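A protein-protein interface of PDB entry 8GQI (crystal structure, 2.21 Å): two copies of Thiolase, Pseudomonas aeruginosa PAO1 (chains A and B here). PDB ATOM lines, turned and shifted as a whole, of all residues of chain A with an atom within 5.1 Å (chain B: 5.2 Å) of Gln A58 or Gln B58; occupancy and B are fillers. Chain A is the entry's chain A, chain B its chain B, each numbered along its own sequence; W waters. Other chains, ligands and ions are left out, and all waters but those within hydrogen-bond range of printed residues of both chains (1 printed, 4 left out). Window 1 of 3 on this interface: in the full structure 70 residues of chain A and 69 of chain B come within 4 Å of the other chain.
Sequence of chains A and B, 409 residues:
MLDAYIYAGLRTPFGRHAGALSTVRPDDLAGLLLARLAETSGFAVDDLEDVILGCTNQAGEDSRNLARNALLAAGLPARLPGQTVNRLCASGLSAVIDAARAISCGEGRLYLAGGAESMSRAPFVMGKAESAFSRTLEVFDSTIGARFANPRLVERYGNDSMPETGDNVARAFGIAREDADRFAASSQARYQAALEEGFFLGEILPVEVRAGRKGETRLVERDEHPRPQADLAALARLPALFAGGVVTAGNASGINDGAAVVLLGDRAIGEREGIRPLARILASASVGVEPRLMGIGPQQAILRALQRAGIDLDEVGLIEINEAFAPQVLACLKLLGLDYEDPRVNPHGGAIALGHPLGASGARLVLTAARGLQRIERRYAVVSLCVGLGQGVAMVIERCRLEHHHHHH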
ATOM      1  N   CYS A  55     -21.937  29.555  18.938  1.00  0.00           N
ATOM      2  CA  CYS A  55     -21.333  30.735  19.623  1.00  0.00           C
ATOM      3  C   CYS A  55     -19.858  30.738  19.290  1.00  0.00           C
ATOM      4  O   CYS A  55     -19.212  29.708  19.522  1.00  0.00           O
ATOM      5  CB  CYS A  55     -21.534  30.674  21.125  1.00  0.00           C
ATOM      6  SG  CYS A  55     -20.934  32.157  21.983  1.00  0.00           S
ATOM      7  N   THR A  56     -19.375  31.805  18.650  1.00  0.00           N
ATOM      8  CA  THR A  56     -17.990  31.872  18.146  1.00  0.00           C
ATOM      9  C   THR A  56     -17.010  32.289  19.251  1.00  0.00           C
ATOM     10  O   THR A  56     -15.830  32.181  18.997  1.00  0.00           O
ATOM     11  CB  THR A  56     -17.847  32.849  16.977  1.00  0.00           C
ATOM     12  OG1 THR A  56     -17.927  34.167  17.538  1.00  0.00           O
ATOM     13  CG2 THR A  56     -18.869  32.592  15.881  1.00  0.00           C
ATOM     14  N   ASN A  57     -17.479  32.714  20.416  1.00  0.00           N
ATOM     15  CA  ASN A  57     -16.642  33.394  21.460  1.00  0.00           C
ATOM     16  C   ASN A  57     -16.460  32.424  22.635  1.00  0.00           C
ATOM     17  O   ASN A  57     -15.498  31.714  22.611  1.00  0.00           O
ATOM     18  CB  ASN A  57     -17.242  34.753  21.860  1.00  0.00           C
ATOM     19  CG  ASN A  57     -16.311  35.565  22.759  1.00  0.00           C
ATOM     20  OD1 ASN A  57     -15.756  35.047  23.717  1.00  0.00           O
ATOM     21  ND2 ASN A  57     -16.050  36.807  22.401  1.00  0.00           N
ATOM     22  N   GLN A  58     -17.432  32.274  23.528  1.00  0.00           N
ATOM     23  CA  GLN A  58     -17.395  31.289  24.653  1.00  0.00           C
ATOM     24  C   GLN A  58     -16.287  31.630  25.689  1.00  0.00           C
ATOM     25  O   GLN A  58     -15.906  30.749  26.458  1.00  0.00           O
ATOM     26  CB  GLN A  58     -17.214  29.877  24.093  1.00  0.00           C
ATOM     27  CG  GLN A  58     -18.231  29.509  23.020  1.00  0.00           C
ATOM     28  CD  GLN A  58     -18.257  28.048  22.654  1.00  0.00           C
ATOM     29  OE1 GLN A  58     -18.284  27.161  23.491  1.00  0.00           O
ATOM     30  NE2 GLN A  58     -18.302  27.796  21.369  1.00  0.00           N
ATOM     31  N   ALA A  59     -15.851  32.894  25.795  1.00  0.00           N
ATOM     32  CA  ALA A  59     -14.862  33.356  26.805  1.00  0.00           C
ATOM     33  C   ALA A  59     -15.553  34.041  27.983  1.00  0.00           C
ATOM     34  O   ALA A  59     -14.862  34.270  29.000  1.00  0.00           O
ATOM     35  CB  ALA A  59     -13.890  34.300  26.149  1.00  0.00           C
ATOM     36  N   GLY A  60     -16.852  34.361  27.864  1.00  0.00           N
ATOM     37  CA  GLY A  60     -17.546  35.341  28.721  1.00  0.00           C
ATOM     38  C   GLY A  60     -18.722  34.755  29.471  1.00  0.00           C
ATOM     39  O   GLY A  60     -18.608  33.659  30.054  1.00  0.00           O
ATOM     40  N   ASP A  62     -20.989  33.586  27.927  1.00  0.00           N
ATOM     41  CA  ASP A  62     -21.336  32.528  26.935  1.00  0.00           C
ATOM     42  C   ASP A  62     -20.388  31.346  27.124  1.00  0.00           C
ATOM     43  O   ASP A  62     -20.376  30.490  26.242  1.00  0.00           O
ATOM     44  CB  ASP A  62     -21.255  33.052  25.488  1.00  0.00           C
ATOM     45  CG  ASP A  62     -19.973  33.808  25.158  1.00  0.00           C
ATOM     46  OD1 ASP A  62     -19.188  34.128  26.116  1.00  0.00           O
ATOM     47  OD2 ASP A  62     -19.781  34.132  23.946  1.00  0.00           O
ATOM     48  N   SER A  63     -19.592  31.328  28.203  1.00  0.00           N
ATOM     49  CA  SER A  63     -18.548  30.294  28.443  1.00  0.00           C
ATOM     50  C   SER A  63     -19.164  29.076  29.113  1.00  0.00           C
ATOM     51  O   SER A  63     -20.309  29.177  29.539  1.00  0.00           O
ATOM     52  CB  SER A  63     -17.408  30.845  29.267  1.00  0.00           C
ATOM     53  OG  SER A  63     -17.786  30.936  30.616  1.00  0.00           O
ATOM     54  N   ARG A  64     -18.417  27.977  29.190  1.00  0.00           N
ATOM     55  CA  ARG A  64     -18.777  26.755  29.963  1.00  0.00           C
ATOM     56  C   ARG A  64     -20.096  26.178  29.448  1.00  0.00           C
ATOM     57  O   ARG A  64     -20.891  25.611  30.275  1.00  0.00           O
ATOM     58  CB  ARG A  64     -18.797  27.071  31.465  1.00  0.00           C
ATOM     59  CG  ARG A  64     -17.442  27.526  31.994  1.00  0.00           C
ATOM     60  CD  ARG A  64     -17.435  27.654  33.498  1.00  0.00           C
ATOM     61  NE  ARG A  64     -17.444  26.375  34.218  1.00  0.00           N
ATOM     62  CZ  ARG A  64     -18.405  25.943  35.044  1.00  0.00           C
ATOM     63  NH1 ARG A  64     -19.486  26.674  35.274  1.00  0.00           N
ATOM     64  NH2 ARG A  64     -18.281  24.768  35.643  1.00  0.00           N
ATOM     65  N   THR A  84     -22.705  23.353  22.720  1.00  0.00           N
ATOM     66  CA  THR A  84     -22.392  24.608  22.052  1.00  0.00           C
ATOM     67  C   THR A  84     -21.439  24.268  20.932  1.00  0.00           C
ATOM     68  O   THR A  84     -20.454  23.536  21.177  1.00  0.00           O
ATOM     69  CB  THR A  84     -21.855  25.668  23.035  1.00  0.00           C
ATOM     70  OG1 THR A  84     -22.815  25.818  24.076  1.00  0.00           O
ATOM     71  CG2 THR A  84     -21.638  26.990  22.339  1.00  0.00           C
ATOM     72  N   VAL A  85     -21.668  24.875  19.789  1.00  0.00           N
ATOM     73  CA  VAL A  85     -20.902  24.557  18.560  1.00  0.00           C
ATOM     74  C   VAL A  85     -20.217  25.822  18.083  1.00  0.00           C
ATOM     75  O   VAL A  85     -20.802  26.870  18.232  1.00  0.00           O
ATOM     76  CB  VAL A  85     -21.864  23.987  17.492  1.00  0.00           C
ATOM     77  CG1 VAL A  85     -21.295  24.088  16.103  1.00  0.00           C
ATOM     78  CG2 VAL A  85     -22.171  22.541  17.820  1.00  0.00           C
ATOM     79  N   ASN A  86     -19.053  25.695  17.453  1.00  0.00           N
ATOM     80  CA  ASN A  86     -18.289  26.852  16.939  1.00  0.00           C
ATOM     81  C   ASN A  86     -17.706  26.501  15.583  1.00  0.00           C
ATOM     82  O   ASN A  86     -16.765  25.707  15.543  1.00  0.00           O
ATOM     83  CB  ASN A  86     -17.174  27.258  17.910  1.00  0.00           C
ATOM     84  CG  ASN A  86     -16.433  28.518  17.551  1.00  0.00           C
ATOM     85  OD1 ASN A  86     -16.582  29.073  16.470  1.00  0.00           O
ATOM     86  ND2 ASN A  86     -15.597  28.979  18.478  1.00  0.00           N
ATOM     87  N   ARG A 147      -6.938  36.568  17.624  1.00  0.00           N
ATOM     88  CA  ARG A 147      -6.294  36.631  18.948  1.00  0.00           C
ATOM     89  C   ARG A 147      -5.432  35.377  19.110  1.00  0.00           C
ATOM     90  O   ARG A 147      -5.881  34.286  18.706  1.00  0.00           O
ATOM     91  CB  ARG A 147      -7.337  36.780  20.054  1.00  0.00           C
ATOM     92  CG  ARG A 147      -8.411  35.705  20.096  1.00  0.00           C
ATOM     93  CD  ARG A 147      -9.365  36.096  21.213  1.00  0.00           C
ATOM     94  NE  ARG A 147     -10.589  35.304  21.308  1.00  0.00           N
ATOM     95  CZ  ARG A 147     -11.608  35.364  20.452  1.00  0.00           C
ATOM     96  NH1 ARG A 147     -11.585  36.167  19.405  1.00  0.00           N
ATOM     97  NH2 ARG A 147     -12.674  34.623  20.671  1.00  0.00           N
ATOM     98  N   CYS B  55     -13.550  21.104  22.784  1.00  0.00           N
ATOM     99  CA  CYS B  55     -12.693  22.031  23.575  1.00  0.00           C
ATOM    100  C   CYS B  55     -13.605  22.805  24.532  1.00  0.00           C
ATOM    101  O   CYS B  55     -14.553  23.396  24.050  1.00  0.00           O
ATOM    102  CB  CYS B  55     -11.934  22.981  22.662  1.00  0.00           C
ATOM    103  SG  CYS B  55     -10.808  24.051  23.601  1.00  0.00           S
ATOM    104  N   THR B  56     -13.388  22.743  25.846  1.00  0.00           N
ATOM    105  CA  THR B  56     -14.309  23.369  26.825  1.00  0.00           C
ATOM    106  C   THR B  56     -14.028  24.856  27.000  1.00  0.00           C
ATOM    107  O   THR B  56     -14.857  25.511  27.582  1.00  0.00           O
ATOM    108  CB  THR B  56     -14.240  22.741  28.217  1.00  0.00           C
ATOM    109  OG1 THR B  56     -12.965  23.048  28.778  1.00  0.00           O
ATOM    110  CG2 THR B  56     -14.513  21.259  28.170  1.00  0.00           C
ATOM    111  N   ASN B  57     -12.934  25.367  26.477  1.00  0.00           N
ATOM    112  CA  ASN B  57     -12.447  26.713  26.828  1.00  0.00           C
ATOM    113  C   ASN B  57     -12.715  27.647  25.650  1.00  0.00           C
ATOM    114  O   ASN B  57     -13.748  28.338  25.664  1.00  0.00           O
ATOM    115  CB  ASN B  57     -10.996  26.611  27.323  1.00  0.00           C
ATOM    116  CG  ASN B  57     -10.450  27.924  27.857  1.00  0.00           C
ATOM    117  OD1 ASN B  57     -10.498  28.948  27.202  1.00  0.00           O
ATOM    118  ND2 ASN B  57      -9.926  27.913  29.061  1.00  0.00           N
ATOM    119  N   GLN B  58     -11.818  27.668  24.675  1.00  0.00           N
ATOM    120  CA  GLN B  58     -11.972  28.382  23.380  1.00  0.00           C
ATOM    121  C   GLN B  58     -11.810  29.896  23.577  1.00  0.00           C
ATOM    122  O   GLN B  58     -12.086  30.657  22.645  1.00  0.00           O
ATOM    123  CB  GLN B  58     -13.295  27.991  22.693  1.00  0.00           C
ATOM    124  CG  GLN B  58     -13.508  26.495  22.499  1.00  0.00           C
ATOM    125  CD  GLN B  58     -14.699  26.209  21.606  1.00  0.00           C
ATOM    126  OE1 GLN B  58     -15.617  25.489  21.985  1.00  0.00           O
ATOM    127  NE2 GLN B  58     -14.736  26.840  20.454  1.00  0.00           N
ATOM    128  N   ALA B  59     -11.181  30.317  24.679  1.00  0.00           N
ATOM    129  CA  ALA B  59     -10.875  31.729  25.004  1.00  0.00           C
ATOM    130  C   ALA B  59      -9.476  32.113  24.525  1.00  0.00           C
ATOM    131  O   ALA B  59      -9.241  33.325  24.371  1.00  0.00           O
ATOM    132  CB  ALA B  59     -11.005  31.929  26.496  1.00  0.00           C
ATOM    133  N   GLY B  60      -8.567  31.139  24.337  1.00  0.00           N
ATOM    134  CA  GLY B  60      -7.132  31.408  24.157  1.00  0.00           C
ATOM    135  C   GLY B  60      -6.572  31.009  22.810  1.00  0.00           C
ATOM    136  O   GLY B  60      -7.000  31.531  21.795  1.00  0.00           O
ATOM    137  N   ASP B  62      -6.838  28.217  21.639  1.00  0.00           N
ATOM    138  CA  ASP B  62      -7.884  27.244  21.263  1.00  0.00           C
ATOM    139  C   ASP B  62      -9.116  28.013  20.772  1.00  0.00           C
ATOM    140  O   ASP B  62     -10.195  27.410  20.696  1.00  0.00           O
ATOM    141  CB  ASP B  62      -8.221  26.353  22.468  1.00  0.00           C
ATOM    142  CG  ASP B  62      -8.600  27.114  23.721  1.00  0.00           C
ATOM    143  OD1 ASP B  62      -8.317  28.333  23.762  1.00  0.00           O
ATOM    144  OD2 ASP B  62      -9.172  26.486  24.682  1.00  0.00           O
ATOM    145  N   SER B  63      -8.976  29.315  20.505  1.00  0.00           N
ATOM    146  CA  SER B  63     -10.124  30.212  20.235  1.00  0.00           C
ATOM    147  C   SER B  63     -10.393  30.297  18.732  1.00  0.00           C
ATOM    148  O   SER B  63      -9.512  29.946  17.930  1.00  0.00           O
ATOM    149  CB  SER B  63      -9.908  31.606  20.840  1.00  0.00           C
ATOM    150  OG  SER B  63      -9.097  32.396  19.994  1.00  0.00           O
ATOM    151  N   ARG B  64     -11.557  30.805  18.359  1.00  0.00           N
ATOM    152  CA  ARG B  64     -11.855  31.079  16.942  1.00  0.00           C
ATOM    153  C   ARG B  64     -11.835  29.778  16.106  1.00  0.00           C
ATOM    154  O   ARG B  64     -11.387  29.855  14.945  1.00  0.00           O
ATOM    155  CB  ARG B  64     -10.846  32.108  16.436  1.00  0.00           C
ATOM    156  CG  ARG B  64     -11.145  33.522  16.918  1.00  0.00           C
ATOM    157  CD  ARG B  64     -10.255  34.541  16.219  1.00  0.00           C
ATOM    158  NE  ARG B  64     -10.807  35.067  14.951  1.00  0.00           N
ATOM    159  CZ  ARG B  64     -10.192  35.044  13.759  1.00  0.00           C
ATOM    160  NH1 ARG B  64      -8.998  34.488  13.622  1.00  0.00           N
ATOM    161  NH2 ARG B  64     -10.779  35.573  12.697  1.00  0.00           N
ATOM    162  N   ASN B  65     -12.314  28.667  16.670  1.00  0.00           N
ATOM    163  CA  ASN B  65     -12.555  27.367  15.970  1.00  0.00           C
ATOM    164  C   ASN B  65     -11.234  26.602  15.882  1.00  0.00           C
ATOM    165  O   ASN B  65     -10.582  26.606  14.810  1.00  0.00           O
ATOM    166  CB  ASN B  65     -13.268  27.521  14.612  1.00  0.00           C
ATOM    167  CG  ASN B  65     -13.608  26.198  13.934  1.00  0.00           C
ATOM    168  OD1 ASN B  65     -13.464  25.118  14.508  1.00  0.00           O
ATOM    169  ND2 ASN B  65     -14.027  26.274  12.679  1.00  0.00           N
ATOM    170  N   THR B  84     -15.630  23.139  16.148  1.00  0.00           N
ATOM    171  CA  THR B  84     -15.302  22.860  17.551  1.00  0.00           C
ATOM    172  C   THR B  84     -16.610  22.730  18.300  1.00  0.00           C
ATOM    173  O   THR B  84     -17.476  23.578  18.113  1.00  0.00           O
ATOM    174  CB  THR B  84     -14.342  23.933  18.082  1.00  0.00           C
ATOM    175  OG1 THR B  84     -13.263  24.009  17.142  1.00  0.00           O
ATOM    176  CG2 THR B  84     -13.792  23.609  19.453  1.00  0.00           C
ATOM    177  N   VAL B  85     -16.620  21.820  19.259  1.00  0.00           N
ATOM    178  CA  VAL B  85     -17.792  21.404  20.044  1.00  0.00           C
ATOM    179  C   VAL B  85     -17.463  21.538  21.537  1.00  0.00           C
ATOM    180  O   VAL B  85     -16.352  21.293  21.911  1.00  0.00           O
ATOM    181  CB  VAL B  85     -18.086  19.965  19.572  1.00  0.00           C
ATOM    182  CG1 VAL B  85     -18.669  19.089  20.636  1.00  0.00           C
ATOM    183  CG2 VAL B  85     -18.961  20.012  18.313  1.00  0.00           C
ATOM    184  N   ASN B  86     -18.444  21.934  22.336  1.00  0.00           N
ATOM    185  CA  ASN B  86     -18.335  22.157  23.786  1.00  0.00           C
ATOM    186  C   ASN B  86     -19.552  21.551  24.449  1.00  0.00           C
ATOM    187  O   ASN B  86     -20.630  22.132  24.368  1.00  0.00           O
ATOM    188  CB  ASN B  86     -18.249  23.637  24.153  1.00  0.00           C
ATOM    189  CG  ASN B  86     -17.771  23.855  25.568  1.00  0.00           C
ATOM    190  OD1 ASN B  86     -17.919  22.960  26.401  1.00  0.00           O
ATOM    191  ND2 ASN B  86     -17.319  25.081  25.865  1.00  0.00           N
ATOM    192  N   ARG B 147     -17.117  30.984  35.734  1.00  0.00           N
ATOM    193  CA  ARG B 147     -16.708  32.382  35.450  1.00  0.00           C
ATOM    194  C   ARG B 147     -17.938  33.113  34.907  1.00  0.00           C
ATOM    195  O   ARG B 147     -18.735  32.487  34.168  1.00  0.00           O
ATOM    196  CB  ARG B 147     -15.506  32.428  34.496  1.00  0.00           C
ATOM    197  CG  ARG B 147     -15.657  31.636  33.202  1.00  0.00           C
ATOM    198  CD  ARG B 147     -14.427  31.837  32.307  1.00  0.00           C
ATOM    199  NE  ARG B 147     -14.264  30.865  31.222  1.00  0.00           N
ATOM    200  CZ  ARG B 147     -14.055  29.557  31.408  1.00  0.00           C
ATOM    201  NH1 ARG B 147     -13.987  29.042  32.623  1.00  0.00           N
ATOM    202  NH2 ARG B 147     -13.926  28.749  30.374  1.00  0.00           N
HETATM  203  O   HOH W   1     -13.758  30.100  28.115  1.00  0.00           O
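Asn A57 touches Gln B58, and with the chains exchanged Gln A58 touches Asn B57. Gln A58 touches Asn B86, and with the chains exchanged Asn A86 touches Gln B58. Thr A84 touches Asn B86, and with the chains exchanged Asn A86 touches Thr B84. Arg A147 touches Ala B59, but with the chains exchanged Ala A59 does not touch Arg B147 (4.1 Å). Positions printed for both chains: 55, 56, 57, 58, 59, 60, 62, 63, 64, 84, 85, 86 and 147. Of the 16 pairs that touch across the chains among the printed residues, 14 have their exchanged pair printed and touching as well.
Asn A57 touches Gln B58. Ala A59 touches Ala B59. Ser A63 touches Arg B147 (OG to CG, 3.4 Å). Arg A64 touches Arg B147. Val B85 touches Thr A84 (CA to O, 3.6 Å). Thr B84 touches Val A85 (O to C, 3.5 Å). Asn A86 touches Asn B65 (O to OD1, 3.5 Å). Ala B59 touches Arg A147 (O to NE, 3.9 Å). OG of Ser B63 touches CG of Arg A147, 3.4 Å away. Arg B64 touches Arg A147.
Gln B58 touches three residues of chain A. Of the printed residues of chain B, Arg A64 touches Arg B147 (3.8 Å). Of the printed residues of chain A, Thr B84 touches Val A85 (3.5 Å) and Asn A86 (2.7 Å). Printed residues of chain A within 4 Å of Arg B64: Arg A147. Of the printed residues of chain B, Asn A86 touches Gln B58 (3.0 Å), Asn B65 (3.5 Å) and Thr B84 (2.7 Å). Asp B62 touches none of the printed residues of chain A. Thr B56 touches none of the printed residues of chain A. The nearest residue of chain B that does not touch Gln A58 is Arg B147 (4.8 Å). The nearest residue of chain A that does not touch Gln B58 is Arg A147 (4.5 Å).
Water W1 lies within hydrogen-bond range of the guanidinium group (NH2) of Arg B147, the backbone carbonyl oxygen (O) of Gln A58 and the backbone carbonyl oxygen (O) of Asn B57.
The side-chain amide oxygen (OE1) of Gln A58 sits at hydrogen-bond distance from the side-chain amide nitrogen (ND2) of Asn B86 (3.3 Å). OE1 of Gln B58 sits close to OE1 of Gln A58 (3.5 Å). N of Asn A86 lies within hydrogen-bond range of O of Thr B84, at 2.7 Å. O of Thr A84 sits at hydrogen-bond distance from N of Asn B86. ND2 of Asn A86 sits close to NE2 of Gln B58, at 3.0 Å. The backbone carbonyl oxygen (O) of Gln A58 lies close to the backbone carbonyl oxygen (O) of Asn B57.
Hydrophobic or aromatic side chains of chain A within 4 Å of the printed part of chain B: Ala A59. Of the 14 printed residues of chain B, 10 touch a printed residue of chain A. Printed residues of chain B that touch a printed residue of chain A: Asn B57, Gln B58, Ala B59, Ser B63, Arg B64, Asn B65, Thr B84, Val B85, Asn B86 and Arg B147. Hydrophobic or aromatic side chains of chain B within 4 Å of the printed part of chain A: Ala B59. Among the printed residues, 16 pairs touch across the chains. Among the printed residues, no Asp or Glu carboxylate lies within 4 Å of a Lys or Arg side-chain nitrogen of the other chain.
The backbone carbonyl oxygen (O) of Val B85 is in hydrogen-bond range of the backbone NH (N) of Cys B55 (2.9 Å). The backbone carbonyl oxygen (O) of Thr A56 sits at hydrogen-bond distance from the side-chain amide nitrogen (ND2) of Asn A86 (3.3 Å). The backbone carbonyl oxygen (O) of Gly B60 lies within hydrogen-bond range of the side-chain hydroxyl (OG) of Ser B63, at 2.9 Å. The backbone carbonyl oxygen (O) of Cys A55 sits at hydrogen-bond distance from the side-chain amide nitrogen (NE2) of Gln A58. OD1 of Asn B65 is in hydrogen-bond range of OG1 of Thr B84. OD1 of Asn A57 sits at hydrogen-bond distance from N of Ala A59, 3.0 Å away.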
